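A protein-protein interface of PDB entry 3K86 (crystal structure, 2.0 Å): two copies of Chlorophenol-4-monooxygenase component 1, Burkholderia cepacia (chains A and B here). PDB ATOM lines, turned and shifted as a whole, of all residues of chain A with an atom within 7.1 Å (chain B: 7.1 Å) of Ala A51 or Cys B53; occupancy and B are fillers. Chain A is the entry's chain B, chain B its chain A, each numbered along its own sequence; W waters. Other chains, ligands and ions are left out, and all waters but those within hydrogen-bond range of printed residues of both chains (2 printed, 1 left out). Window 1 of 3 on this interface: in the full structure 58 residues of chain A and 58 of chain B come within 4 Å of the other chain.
O of Val B55 sits close to ND1 of His A145 (3.5 Å).
The backbone carbonyl oxygen (O) of Cys B53 is in hydrogen-bond range of the backbone NH (N) of Leu B63 (2.8 Å). The backbone NH of Val B55 sits at hydrogen-bond distance from the backbone carbonyl oxygen of Thr B61 (2.8 Å). SG of Cys A49 is in hydrogen-bond range of O of Ala A51, 3.5 Å away. SG of Cys A49 sits at hydrogen-bond distance from O of Cys A65 (3.5 Å). O of Ala A51 lies within hydrogen-bond range of N of Cys A65, 3.0 Å away. The backbone NH (N) of Leu A63 lies within hydrogen-bond range of the backbone carbonyl oxygen (O) of Cys A53 (2.9 Å).
Among the printed residues, merely in contact across the chains: Phe A22 with Cys B56 (3.3 Å), Ala A51 with Ser B54 (3.4 Å), Leu A26 with Ser B54 (3.4 Å), Phe A22 with Thr B61 (3.5 Å), Leu A63 with Leu B63 (3.7 Å), Phe A22 with Val B62 (3.7 Å), Cys A53 with Cys B65 (3.8 Å), Val A147 with Val B55 (3.8 Å), Ala A51 with Cys B53 (3.9 Å), Cys A53 with Ala B51 (3.9 Å), Cys A65 with Cys B53 (3.95 Å), Leu A63 with Cys B53 (3.97 Å), Phe A22 with Ser B54 (3.97 Å) and Cys A65 with Ser B54 (3.97 Å).
Ala A51 touches Cys B53, and with the chains exchanged Cys A53 touches Ala B51. Cys A53 touches Cys B65, and with the chains exchanged Cys A65 touches Cys B53. Leu A63 touches Cys B53, but with the chains exchanged Cys A53 does not touch Leu B63 (4.01 Å). Leu A63 touches its own counterpart, Leu B63. Of the 15 pairs that touch across the chains among the printed residues, 5 have their exchanged pair printed and touching as well.
Water W1 bridges the side-chain hydroxyl of Ser A50 (2.8 Å) and the side-chain hydroxyl of Ser B54 (2.8 Å). Water W2 lies within hydrogen-bond range of the backbone NH of Ser B54 (2.9 Å) and the backbone carbonyl oxygen of Ser A50 (3.1 Å).
Ala A51 touches just these residues of chain B: Cys B53 (3.9 Å) and Ser B54 (3.4 Å). Cys B53 touches three residues of chain A. Printed residues of chain A within 4 Å of Val B62: Phe A22 (3.7 Å). Printed residues of chain A within 4 Å of Cys B56: Phe A22 (3.3 Å). Of the printed residues of chain A, Leu B63 touches Leu A63 (3.7 Å). Of the printed residues of chain B, Phe A22 touches Ser B54 (3.97 Å), Cys B56 (3.3 Å), Thr B61 (3.5 Å) and Val B62 (3.7 Å). Of the printed residues of chain B, Cys A53 touches Ala B51 and Cys B65. Pro B32 touches none of the printed residues of chain A. Val B52 touches none of the printed residues of chain A. The nearest residue of chain B that does not touch Ala A51 is Val B55 (5.6 Å). The nearest residue of chain A that does not touch Cys B53 is Val A52 (4.1 Å). The nearest printed residue of chain A that does not touch Thr B61 is Leu A26 (6.3 Å).
Of the 18 printed residues of chain A, 8 touch a printed residue of chain B. Hydrophobic or aromatic side chains of chain A within 4 Å of the printed part of chain B: Phe A22, Leu A26, Ala A51, Leu A63, His A145 and Val A147. Along chain A the printed residues that touch a printed residue of chain B span positions 22 to 147. Among the printed residues, no Asp or Glu carboxylate lies within 4 Å of a Lys or Arg side-chain nitrogen of the other chain.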
ATOM      1  N   PHE A  22     -21.833 -12.329  -6.198  1.00  0.00           N
ATOM      2  CA  PHE A  22     -21.250 -13.226  -5.194  1.00  0.00           C
ATOM      3  C   PHE A  22     -22.249 -14.309  -4.817  1.00  0.00           C
ATOM      4  O   PHE A  22     -21.879 -15.461  -4.768  1.00  0.00           O
ATOM      5  CB  PHE A  22     -20.912 -12.377  -3.956  1.00  0.00           C
ATOM      6  CG  PHE A  22     -20.327 -13.137  -2.810  1.00  0.00           C
ATOM      7  CD1 PHE A  22     -21.056 -13.310  -1.629  1.00  0.00           C
ATOM      8  CD2 PHE A  22     -19.025 -13.603  -2.867  1.00  0.00           C
ATOM      9  CE1 PHE A  22     -20.498 -13.962  -0.534  1.00  0.00           C
ATOM     10  CE2 PHE A  22     -18.445 -14.256  -1.763  1.00  0.00           C
ATOM     11  CZ  PHE A  22     -19.183 -14.440  -0.604  1.00  0.00           C
ATOM     12  N   LEU A  26     -21.839 -18.409  -5.411  1.00  0.00           N
ATOM     13  CA  LEU A  26     -21.880 -19.378  -4.323  1.00  0.00           C
ATOM     14  C   LEU A  26     -22.851 -20.541  -4.595  1.00  0.00           C
ATOM     15  O   LEU A  26     -22.612 -21.662  -4.108  1.00  0.00           O
ATOM     16  CB  LEU A  26     -22.237 -18.700  -2.980  1.00  0.00           C
ATOM     17  CG  LEU A  26     -21.126 -17.781  -2.407  1.00  0.00           C
ATOM     18  CD1 LEU A  26     -21.608 -17.192  -1.050  1.00  0.00           C
ATOM     19  CD2 LEU A  26     -19.842 -18.576  -2.240  1.00  0.00           C
ATOM     20  N   THR A  31     -21.583 -27.360  -0.649  1.00  0.00           N
ATOM     21  CA  THR A  31     -21.257 -27.336   0.781  1.00  0.00           C
ATOM     22  C   THR A  31     -21.880 -28.543   1.462  1.00  0.00           C
ATOM     23  O   THR A  31     -22.902 -29.036   1.001  1.00  0.00           O
ATOM     24  CB  THR A  31     -21.868 -26.114   1.485  1.00  0.00           C
ATOM     25  OG1 THR A  31     -23.273 -26.051   1.227  1.00  0.00           O
ATOM     26  CG2 THR A  31     -21.192 -24.778   1.015  1.00  0.00           C
ATOM     27  N   PRO A  32     -21.274 -29.020   2.567  1.00  0.00           N
ATOM     28  CA  PRO A  32     -21.951 -30.050   3.360  1.00  0.00           C
ATOM     29  C   PRO A  32     -23.128 -29.350   4.061  1.00  0.00           C
ATOM     30  O   PRO A  32     -23.090 -28.136   4.287  1.00  0.00           O
ATOM     31  CB  PRO A  32     -20.884 -30.439   4.393  1.00  0.00           C
ATOM     32  CG  PRO A  32     -20.107 -29.130   4.570  1.00  0.00           C
ATOM     33  CD  PRO A  32     -19.953 -28.689   3.128  1.00  0.00           C
ATOM     34  N   THR A  34     -25.040 -28.700   7.453  1.00  0.00           N
ATOM     35  CA  THR A  34     -24.953 -28.919   8.898  1.00  0.00           C
ATOM     36  C   THR A  34     -26.104 -28.262   9.631  1.00  0.00           C
ATOM     37  O   THR A  34     -26.763 -27.359   9.129  1.00  0.00           O
ATOM     38  CB  THR A  34     -23.627 -28.389   9.534  1.00  0.00           C
ATOM     39  OG1 THR A  34     -23.705 -26.972   9.654  1.00  0.00           O
ATOM     40  CG2 THR A  34     -22.402 -28.738   8.672  1.00  0.00           C
ATOM     41  N   VAL A  36     -26.384 -26.336  13.369  1.00  0.00           N
ATOM     42  CA  VAL A  36     -25.637 -25.850  14.511  1.00  0.00           C
ATOM     43  C   VAL A  36     -26.695 -25.698  15.588  1.00  0.00           C
ATOM     44  O   VAL A  36     -27.726 -25.082  15.349  1.00  0.00           O
ATOM     45  CB  VAL A  36     -24.963 -24.511  14.189  1.00  0.00           C
ATOM     46  CG1 VAL A  36     -24.369 -23.852  15.493  1.00  0.00           C
ATOM     47  CG2 VAL A  36     -23.811 -24.788  13.106  1.00  0.00           C
ATOM     48  N   THR A  48     -29.780 -24.251  10.322  1.00  0.00           N
ATOM     49  CA  THR A  48     -28.988 -24.876   9.291  1.00  0.00           C
ATOM     50  C   THR A  48     -27.811 -23.936   8.918  1.00  0.00           C
ATOM     51  O   THR A  48     -27.965 -22.715   8.925  1.00  0.00           O
ATOM     52  CB  THR A  48     -29.920 -25.193   8.085  1.00  0.00           C
ATOM     53  OG1 THR A  48     -29.316 -26.169   7.244  1.00  0.00           O
ATOM     54  CG2 THR A  48     -30.115 -23.957   7.299  1.00  0.00           C
ATOM     55  N   CYS A  49     -26.639 -24.492   8.606  1.00  0.00           N
ATOM     56  CA  CYS A  49     -25.464 -23.659   8.354  1.00  0.00           C
ATOM     57  C   CYS A  49     -24.612 -24.249   7.237  1.00  0.00           C
ATOM     58  O   CYS A  49     -24.161 -25.394   7.319  1.00  0.00           O
ATOM     59  CB  CYS A  49     -24.634 -23.474   9.640  1.00  0.00           C
ATOM     60  SG  CYS A  49     -23.170 -22.416   9.438  1.00  0.00           S
ATOM     61  N   SER A  50     -24.409 -23.463   6.187  1.00  0.00           N
ATOM     62  CA  SER A  50     -23.648 -23.927   5.031  1.00  0.00           C
ATOM     63  C   SER A  50     -22.256 -23.323   5.026  1.00  0.00           C
ATOM     64  O   SER A  50     -21.585 -23.351   3.994  1.00  0.00           O
ATOM     65  CB  SER A  50     -24.352 -23.522   3.720  1.00  0.00           C
ATOM     66  OG  SER A  50     -24.540 -22.100   3.646  1.00  0.00           O
ATOM     67  N   ALA A  51     -21.832 -22.746   6.153  1.00  0.00           N
ATOM     68  CA  ALA A  51     -20.501 -22.120   6.173  1.00  0.00           C
ATOM     69  C   ALA A  51     -19.788 -22.582   7.408  1.00  0.00           C
ATOM     70  O   ALA A  51     -19.859 -21.934   8.483  1.00  0.00           O
ATOM     71  CB  ALA A  51     -20.667 -20.625   6.150  1.00  0.00           C
ATOM     72  N   VAL A  52     -19.173 -23.751   7.297  1.00  0.00           N
ATOM     73  CA  VAL A  52     -18.445 -24.343   8.437  1.00  0.00           C
ATOM     74  C   VAL A  52     -17.175 -24.896   7.882  1.00  0.00           C
ATOM     75  O   VAL A  52     -17.150 -25.328   6.720  1.00  0.00           O
ATOM     76  CB  VAL A  52     -19.227 -25.516   9.168  1.00  0.00           C
ATOM     77  CG1 VAL A  52     -20.663 -25.130   9.430  1.00  0.00           C
ATOM     78  CG2 VAL A  52     -19.223 -26.725   8.371  1.00  0.00           C
ATOM     79  N   CYS A  53     -16.101 -24.828   8.659  1.00  0.00           N
ATOM     80  CA  CYS A  53     -14.906 -25.560   8.312  1.00  0.00           C
ATOM     81  C   CYS A  53     -13.993 -25.839   9.510  1.00  0.00           C
ATOM     82  O   CYS A  53     -14.162 -25.301  10.613  1.00  0.00           O
ATOM     83  CB  CYS A  53     -14.168 -24.883   7.166  1.00  0.00           C
ATOM     84  SG  CYS A  53     -13.379 -23.324   7.600  1.00  0.00           S
ATOM     85  N   LEU A  63     -14.842 -23.499  12.769  1.00  0.00           N
ATOM     86  CA  LEU A  63     -15.550 -22.221  12.747  1.00  0.00           C
ATOM     87  C   LEU A  63     -16.853 -22.370  11.962  1.00  0.00           C
ATOM     88  O   LEU A  63     -17.011 -23.269  11.129  1.00  0.00           O
ATOM     89  CB  LEU A  63     -14.651 -21.101  12.182  1.00  0.00           C
ATOM     90  CG  LEU A  63     -14.188 -21.151  10.714  1.00  0.00           C
ATOM     91  CD1 LEU A  63     -15.375 -20.917   9.765  1.00  0.00           C
ATOM     92  CD2 LEU A  63     -13.104 -20.041  10.454  1.00  0.00           C
ATOM     93  N   LEU A  64     -17.796 -21.488  12.255  1.00  0.00           N
ATOM     94  CA  LEU A  64     -19.029 -21.473  11.543  1.00  0.00           C
ATOM     95  C   LEU A  64     -19.411 -20.004  11.457  1.00  0.00           C
ATOM     96  O   LEU A  64     -19.094 -19.206  12.351  1.00  0.00           O
ATOM     97  CB  LEU A  64     -20.072 -22.320  12.275  1.00  0.00           C
ATOM     98  CG  LEU A  64     -20.231 -21.986  13.748  1.00  0.00           C
ATOM     99  CD1 LEU A  64     -21.565 -21.294  14.006  1.00  0.00           C
ATOM    100  CD2 LEU A  64     -20.155 -23.251  14.526  1.00  0.00           C
ATOM    101  N   CYS A  65     -20.066 -19.652  10.366  1.00  0.00           N
ATOM    102  CA  CYS A  65     -20.469 -18.283  10.125  1.00  0.00           C
ATOM    103  C   CYS A  65     -21.966 -18.256  10.086  1.00  0.00           C
ATOM    104  O   CYS A  65     -22.593 -18.961   9.263  1.00  0.00           O
ATOM    105  CB  CYS A  65     -19.942 -17.829   8.746  1.00  0.00           C
ATOM    106  SG  CYS A  65     -18.132 -17.965   8.627  1.00  0.00           S
ATOM    107  N   ILE A  66     -22.555 -17.411  10.931  1.00  0.00           N
ATOM    108  CA  ILE A  66     -24.011 -17.339  10.966  1.00  0.00           C
ATOM    109  C   ILE A  66     -24.449 -15.903  10.984  1.00  0.00           C
ATOM    110  O   ILE A  66     -23.797 -15.041  11.582  1.00  0.00           O
ATOM    111  CB  ILE A  66     -24.606 -18.066  12.148  1.00  0.00           C
ATOM    112  CG1 ILE A  66     -24.001 -17.525  13.445  1.00  0.00           C
ATOM    113  CG2 ILE A  66     -24.365 -19.617  12.037  1.00  0.00           C
ATOM    114  CD1 ILE A  66     -24.633 -18.268  14.672  1.00  0.00           C
ATOM    115  N   HIS A 145     -22.388 -11.227   9.403  1.00  0.00           N
ATOM    116  CA  HIS A 145     -22.278 -12.515  10.087  1.00  0.00           C
ATOM    117  C   HIS A 145     -21.326 -12.511  11.276  1.00  0.00           C
ATOM    118  O   HIS A 145     -20.366 -11.742  11.318  1.00  0.00           O
ATOM    119  CB  HIS A 145     -21.787 -13.594   9.109  1.00  0.00           C
ATOM    120  CG  HIS A 145     -22.868 -14.130   8.222  1.00  0.00           C
ATOM    121  ND1 HIS A 145     -23.628 -13.311   7.410  1.00  0.00           N
ATOM    122  CD2 HIS A 145     -23.298 -15.397   8.004  1.00  0.00           C
ATOM    123  CE1 HIS A 145     -24.520 -14.058   6.761  1.00  0.00           C
ATOM    124  NE2 HIS A 145     -24.314 -15.323   7.076  1.00  0.00           N
ATOM    125  N   VAL A 147     -18.544 -14.834  12.899  1.00  0.00           N
ATOM    126  CA  VAL A 147     -17.647 -15.951  12.634  1.00  0.00           C
ATOM    127  C   VAL A 147     -17.240 -16.507  13.977  1.00  0.00           C
ATOM    128  O   VAL A 147     -16.477 -15.866  14.756  1.00  0.00           O
ATOM    129  CB  VAL A 147     -16.422 -15.520  11.824  1.00  0.00           C
ATOM    130  CG1 VAL A 147     -15.517 -16.761  11.539  1.00  0.00           C
ATOM    131  CG2 VAL A 147     -16.900 -14.809  10.511  1.00  0.00           C
ATOM    132  N   PRO B  32     -15.935 -29.487  -0.085  1.00  0.00           N
ATOM    133  CA  PRO B  32     -15.595 -29.202  -1.475  1.00  0.00           C
ATOM    134  C   PRO B  32     -14.085 -29.238  -1.564  1.00  0.00           C
ATOM    135  O   PRO B  32     -13.426 -29.236  -0.547  1.00  0.00           O
ATOM    136  CB  PRO B  32     -16.064 -27.753  -1.635  1.00  0.00           C
ATOM    137  CG  PRO B  32     -15.920 -27.180  -0.236  1.00  0.00           C
ATOM    138  CD  PRO B  32     -16.448 -28.291   0.602  1.00  0.00           C
ATOM    139  N   SER B  50      -9.302 -27.465   1.595  1.00  0.00           N
ATOM    140  CA  SER B  50     -10.681 -27.856   1.777  1.00  0.00           C
ATOM    141  C   SER B  50     -11.294 -27.145   2.973  1.00  0.00           C
ATOM    142  O   SER B  50     -12.426 -27.388   3.269  1.00  0.00           O
ATOM    143  CB  SER B  50     -10.798 -29.365   1.994  1.00  0.00           C
ATOM    144  OG  SER B  50      -9.992 -29.744   3.099  1.00  0.00           O
ATOM    145  N   ALA B  51     -10.567 -26.257   3.640  1.00  0.00           N
ATOM    146  CA  ALA B  51     -11.145 -25.494   4.742  1.00  0.00           C
ATOM    147  C   ALA B  51     -11.481 -24.092   4.230  1.00  0.00           C
ATOM    148  O   ALA B  51     -10.702 -23.134   4.427  1.00  0.00           O
ATOM    149  CB  ALA B  51     -10.104 -25.418   5.909  1.00  0.00           C
ATOM    150  N   VAL B  52     -12.618 -23.964   3.560  1.00  0.00           N
ATOM    151  CA  VAL B  52     -12.977 -22.699   2.896  1.00  0.00           C
ATOM    152  C   VAL B  52     -14.459 -22.465   3.130  1.00  0.00           C
ATOM    153  O   VAL B  52     -15.211 -23.434   3.116  1.00  0.00           O
ATOM    154  CB  VAL B  52     -12.746 -22.749   1.325  1.00  0.00           C
ATOM    155  CG1 VAL B  52     -13.323 -21.521   0.677  1.00  0.00           C
ATOM    156  CG2 VAL B  52     -11.250 -22.835   0.943  1.00  0.00           C
ATOM    157  N   CYS B  53     -14.905 -21.232   3.355  1.00  0.00           N
ATOM    158  CA  CYS B  53     -16.344 -20.991   3.296  1.00  0.00           C
ATOM    159  C   CYS B  53     -16.662 -19.542   3.017  1.00  0.00           C
ATOM    160  O   CYS B  53     -15.776 -18.676   3.130  1.00  0.00           O
ATOM    161  CB  CYS B  53     -17.064 -21.486   4.553  1.00  0.00           C
ATOM    162  SG  CYS B  53     -16.649 -20.545   6.026  1.00  0.00           S
ATOM    163  N   SER B  54     -17.905 -19.260   2.617  1.00  0.00           N
ATOM    164  CA  SER B  54     -18.316 -17.869   2.484  1.00  0.00           C
ATOM    165  C   SER B  54     -18.585 -17.290   3.851  1.00  0.00           C
ATOM    166  O   SER B  54     -19.054 -17.968   4.761  1.00  0.00           O
ATOM    167  CB  SER B  54     -19.597 -17.665   1.670  1.00  0.00           C
ATOM    168  OG  SER B  54     -20.604 -18.482   2.174  1.00  0.00           O
ATOM    169  N   VAL B  55     -18.332 -16.002   3.963  1.00  0.00           N
ATOM    170  CA  VAL B  55     -18.562 -15.306   5.230  1.00  0.00           C
ATOM    171  C   VAL B  55     -19.815 -14.422   5.138  1.00  0.00           C
ATOM    172  O   VAL B  55     -20.741 -14.581   5.925  1.00  0.00           O
ATOM    173  CB  VAL B  55     -17.305 -14.505   5.606  1.00  0.00           C
ATOM    174  CG1 VAL B  55     -17.542 -13.661   6.893  1.00  0.00           C
ATOM    175  CG2 VAL B  55     -16.130 -15.484   5.821  1.00  0.00           C
ATOM    176  N   CYS B  56     -19.848 -13.496   4.187  1.00  0.00           N
ATOM    177  CA  CYS B  56     -20.952 -12.492   4.112  1.00  0.00           C
ATOM    178  C   CYS B  56     -20.938 -11.916   2.700  1.00  0.00           C
ATOM    179  O   CYS B  56     -19.918 -11.989   2.010  1.00  0.00           O
ATOM    180  CB  CYS B  56     -20.783 -11.332   5.113  1.00  0.00           C
ATOM    181  SG  CYS B  56     -19.162 -10.379   4.985  1.00  0.00           S
ATOM    182  N   THR B  61     -17.160 -11.680   0.945  1.00  0.00           N
ATOM    183  CA  THR B  61     -15.991 -12.126   1.687  1.00  0.00           C
ATOM    184  C   THR B  61     -16.091 -13.618   1.868  1.00  0.00           C
ATOM    185  O   THR B  61     -17.175 -14.159   2.204  1.00  0.00           O
ATOM    186  CB  THR B  61     -15.944 -11.487   3.116  1.00  0.00           C
ATOM    187  OG1 THR B  61     -15.892 -10.065   2.986  1.00  0.00           O
ATOM    188  CG2 THR B  61     -14.673 -11.961   3.884  1.00  0.00           C
ATOM    189  N   VAL B  62     -14.984 -14.279   1.581  1.00  0.00           N
ATOM    190  CA  VAL B  62     -14.822 -15.689   1.869  1.00  0.00           C
ATOM    191  C   VAL B  62     -13.660 -15.821   2.877  1.00  0.00           C
ATOM    192  O   VAL B  62     -12.867 -14.869   3.100  1.00  0.00           O
ATOM    193  CB  VAL B  62     -14.529 -16.487   0.576  1.00  0.00           C
ATOM    194  CG1 VAL B  62     -15.702 -16.315  -0.413  1.00  0.00           C
ATOM    195  CG2 VAL B  62     -13.218 -16.038  -0.091  1.00  0.00           C
ATOM    196  N   LEU B  63     -13.532 -16.982   3.486  1.00  0.00           N
ATOM    197  CA  LEU B  63     -12.312 -17.254   4.234  1.00  0.00           C
ATOM    198  C   LEU B  63     -11.725 -18.619   3.847  1.00  0.00           C
ATOM    199  O   LEU B  63     -12.424 -19.508   3.326  1.00  0.00           O
ATOM    200  CB  LEU B  63     -12.566 -17.125   5.755  1.00  0.00           C
ATOM    201  CG  LEU B  63     -13.553 -18.123   6.420  1.00  0.00           C
ATOM    202  CD1 LEU B  63     -12.868 -19.509   6.492  1.00  0.00           C
ATOM    203  CD2 LEU B  63     -13.934 -17.579   7.870  1.00  0.00           C
ATOM    204  N   LEU B  64     -10.437 -18.787   4.101  1.00  0.00           N
ATOM    205  CA  LEU B  64      -9.777 -20.041   3.846  1.00  0.00           C
ATOM    206  C   LEU B  64      -8.756 -20.226   4.955  1.00  0.00           C
ATOM    207  O   LEU B  64      -8.175 -19.235   5.431  1.00  0.00           O
ATOM    208  CB  LEU B  64      -9.079 -19.994   2.472  1.00  0.00           C
ATOM    209  CG  LEU B  64      -8.143 -18.818   2.263  1.00  0.00           C
ATOM    210  CD1 LEU B  64      -6.698 -19.276   2.180  1.00  0.00           C
ATOM    211  CD2 LEU B  64      -8.541 -18.080   0.974  1.00  0.00           C
ATOM    212  N   CYS B  65      -8.537 -21.464   5.381  1.00  0.00           N
ATOM    213  CA  CYS B  65      -7.635 -21.703   6.527  1.00  0.00           C
ATOM    214  C   CYS B  65      -6.474 -22.528   6.021  1.00  0.00           C
ATOM    215  O   CYS B  65      -6.693 -23.620   5.512  1.00  0.00           O
ATOM    216  CB  CYS B  65      -8.362 -22.521   7.620  1.00  0.00           C
ATOM    217  SG  CYS B  65      -9.951 -21.734   8.136  1.00  0.00           S
ATOM    218  N   VAL B  84      -9.537 -18.288  -5.167  1.00  0.00           N
ATOM    219  CA  VAL B  84     -10.083 -19.495  -4.577  1.00  0.00           C
ATOM    220  C   VAL B  84     -10.847 -20.174  -5.710  1.00  0.00           C
ATOM    221  O   VAL B  84     -11.712 -19.557  -6.332  1.00  0.00           O
ATOM    222  CB  VAL B  84     -11.089 -19.182  -3.425  1.00  0.00           C
ATOM    223  CG1 VAL B  84     -11.571 -20.488  -2.793  1.00  0.00           C
ATOM    224  CG2 VAL B  84     -10.426 -18.264  -2.388  1.00  0.00           C
ATOM    225  N   TRP B  86     -13.009 -23.456  -6.728  1.00  0.00           N
ATOM    226  CA  TRP B  86     -13.742 -24.675  -6.389  1.00  0.00           C
ATOM    227  C   TRP B  86     -13.675 -25.605  -7.593  1.00  0.00           C
ATOM    228  O   TRP B  86     -14.094 -25.257  -8.701  1.00  0.00           O
ATOM    229  CB  TRP B  86     -15.199 -24.366  -6.092  1.00  0.00           C
ATOM    230  CG  TRP B  86     -15.486 -23.815  -4.689  1.00  0.00           C
ATOM    231  CD1 TRP B  86     -16.016 -24.507  -3.621  1.00  0.00           C
ATOM    232  CD2 TRP B  86     -15.341 -22.455  -4.251  1.00  0.00           C
ATOM    233  NE1 TRP B  86     -16.164 -23.665  -2.538  1.00  0.00           N
ATOM    234  CE2 TRP B  86     -15.754 -22.410  -2.895  1.00  0.00           C
ATOM    235  CE3 TRP B  86     -14.841 -21.287  -4.849  1.00  0.00           C
ATOM    236  CZ2 TRP B  86     -15.721 -21.226  -2.148  1.00  0.00           C
ATOM    237  CZ3 TRP B  86     -14.818 -20.113  -4.101  1.00  0.00           C
ATOM    238  CH2 TRP B  86     -15.266 -20.091  -2.763  1.00  0.00           C
ATOM    239  N   ILE B 148      -7.620 -16.648   6.652  1.00  0.00           N
ATOM    240  CA  ILE B 148      -7.453 -15.489   5.793  1.00  0.00           C
ATOM    241  C   ILE B 148      -8.830 -15.124   5.247  1.00  0.00           C
ATOM    242  O   ILE B 148      -9.474 -15.961   4.589  1.00  0.00           O
ATOM    243  CB  ILE B 148      -6.504 -15.830   4.607  1.00  0.00           C
ATOM    244  CG1 ILE B 148      -5.115 -16.213   5.153  1.00  0.00           C
ATOM    245  CG2 ILE B 148      -6.472 -14.656   3.604  1.00  0.00           C
ATOM    246  CD1 ILE B 148      -4.133 -16.821   4.123  1.00  0.00           C
HETATM  247  O   HOH W   1     -22.616 -20.409   2.528  1.00  0.00           O
HETATM  248  O   HOH W   2     -19.574 -21.570   2.442  1.00  0.00           O
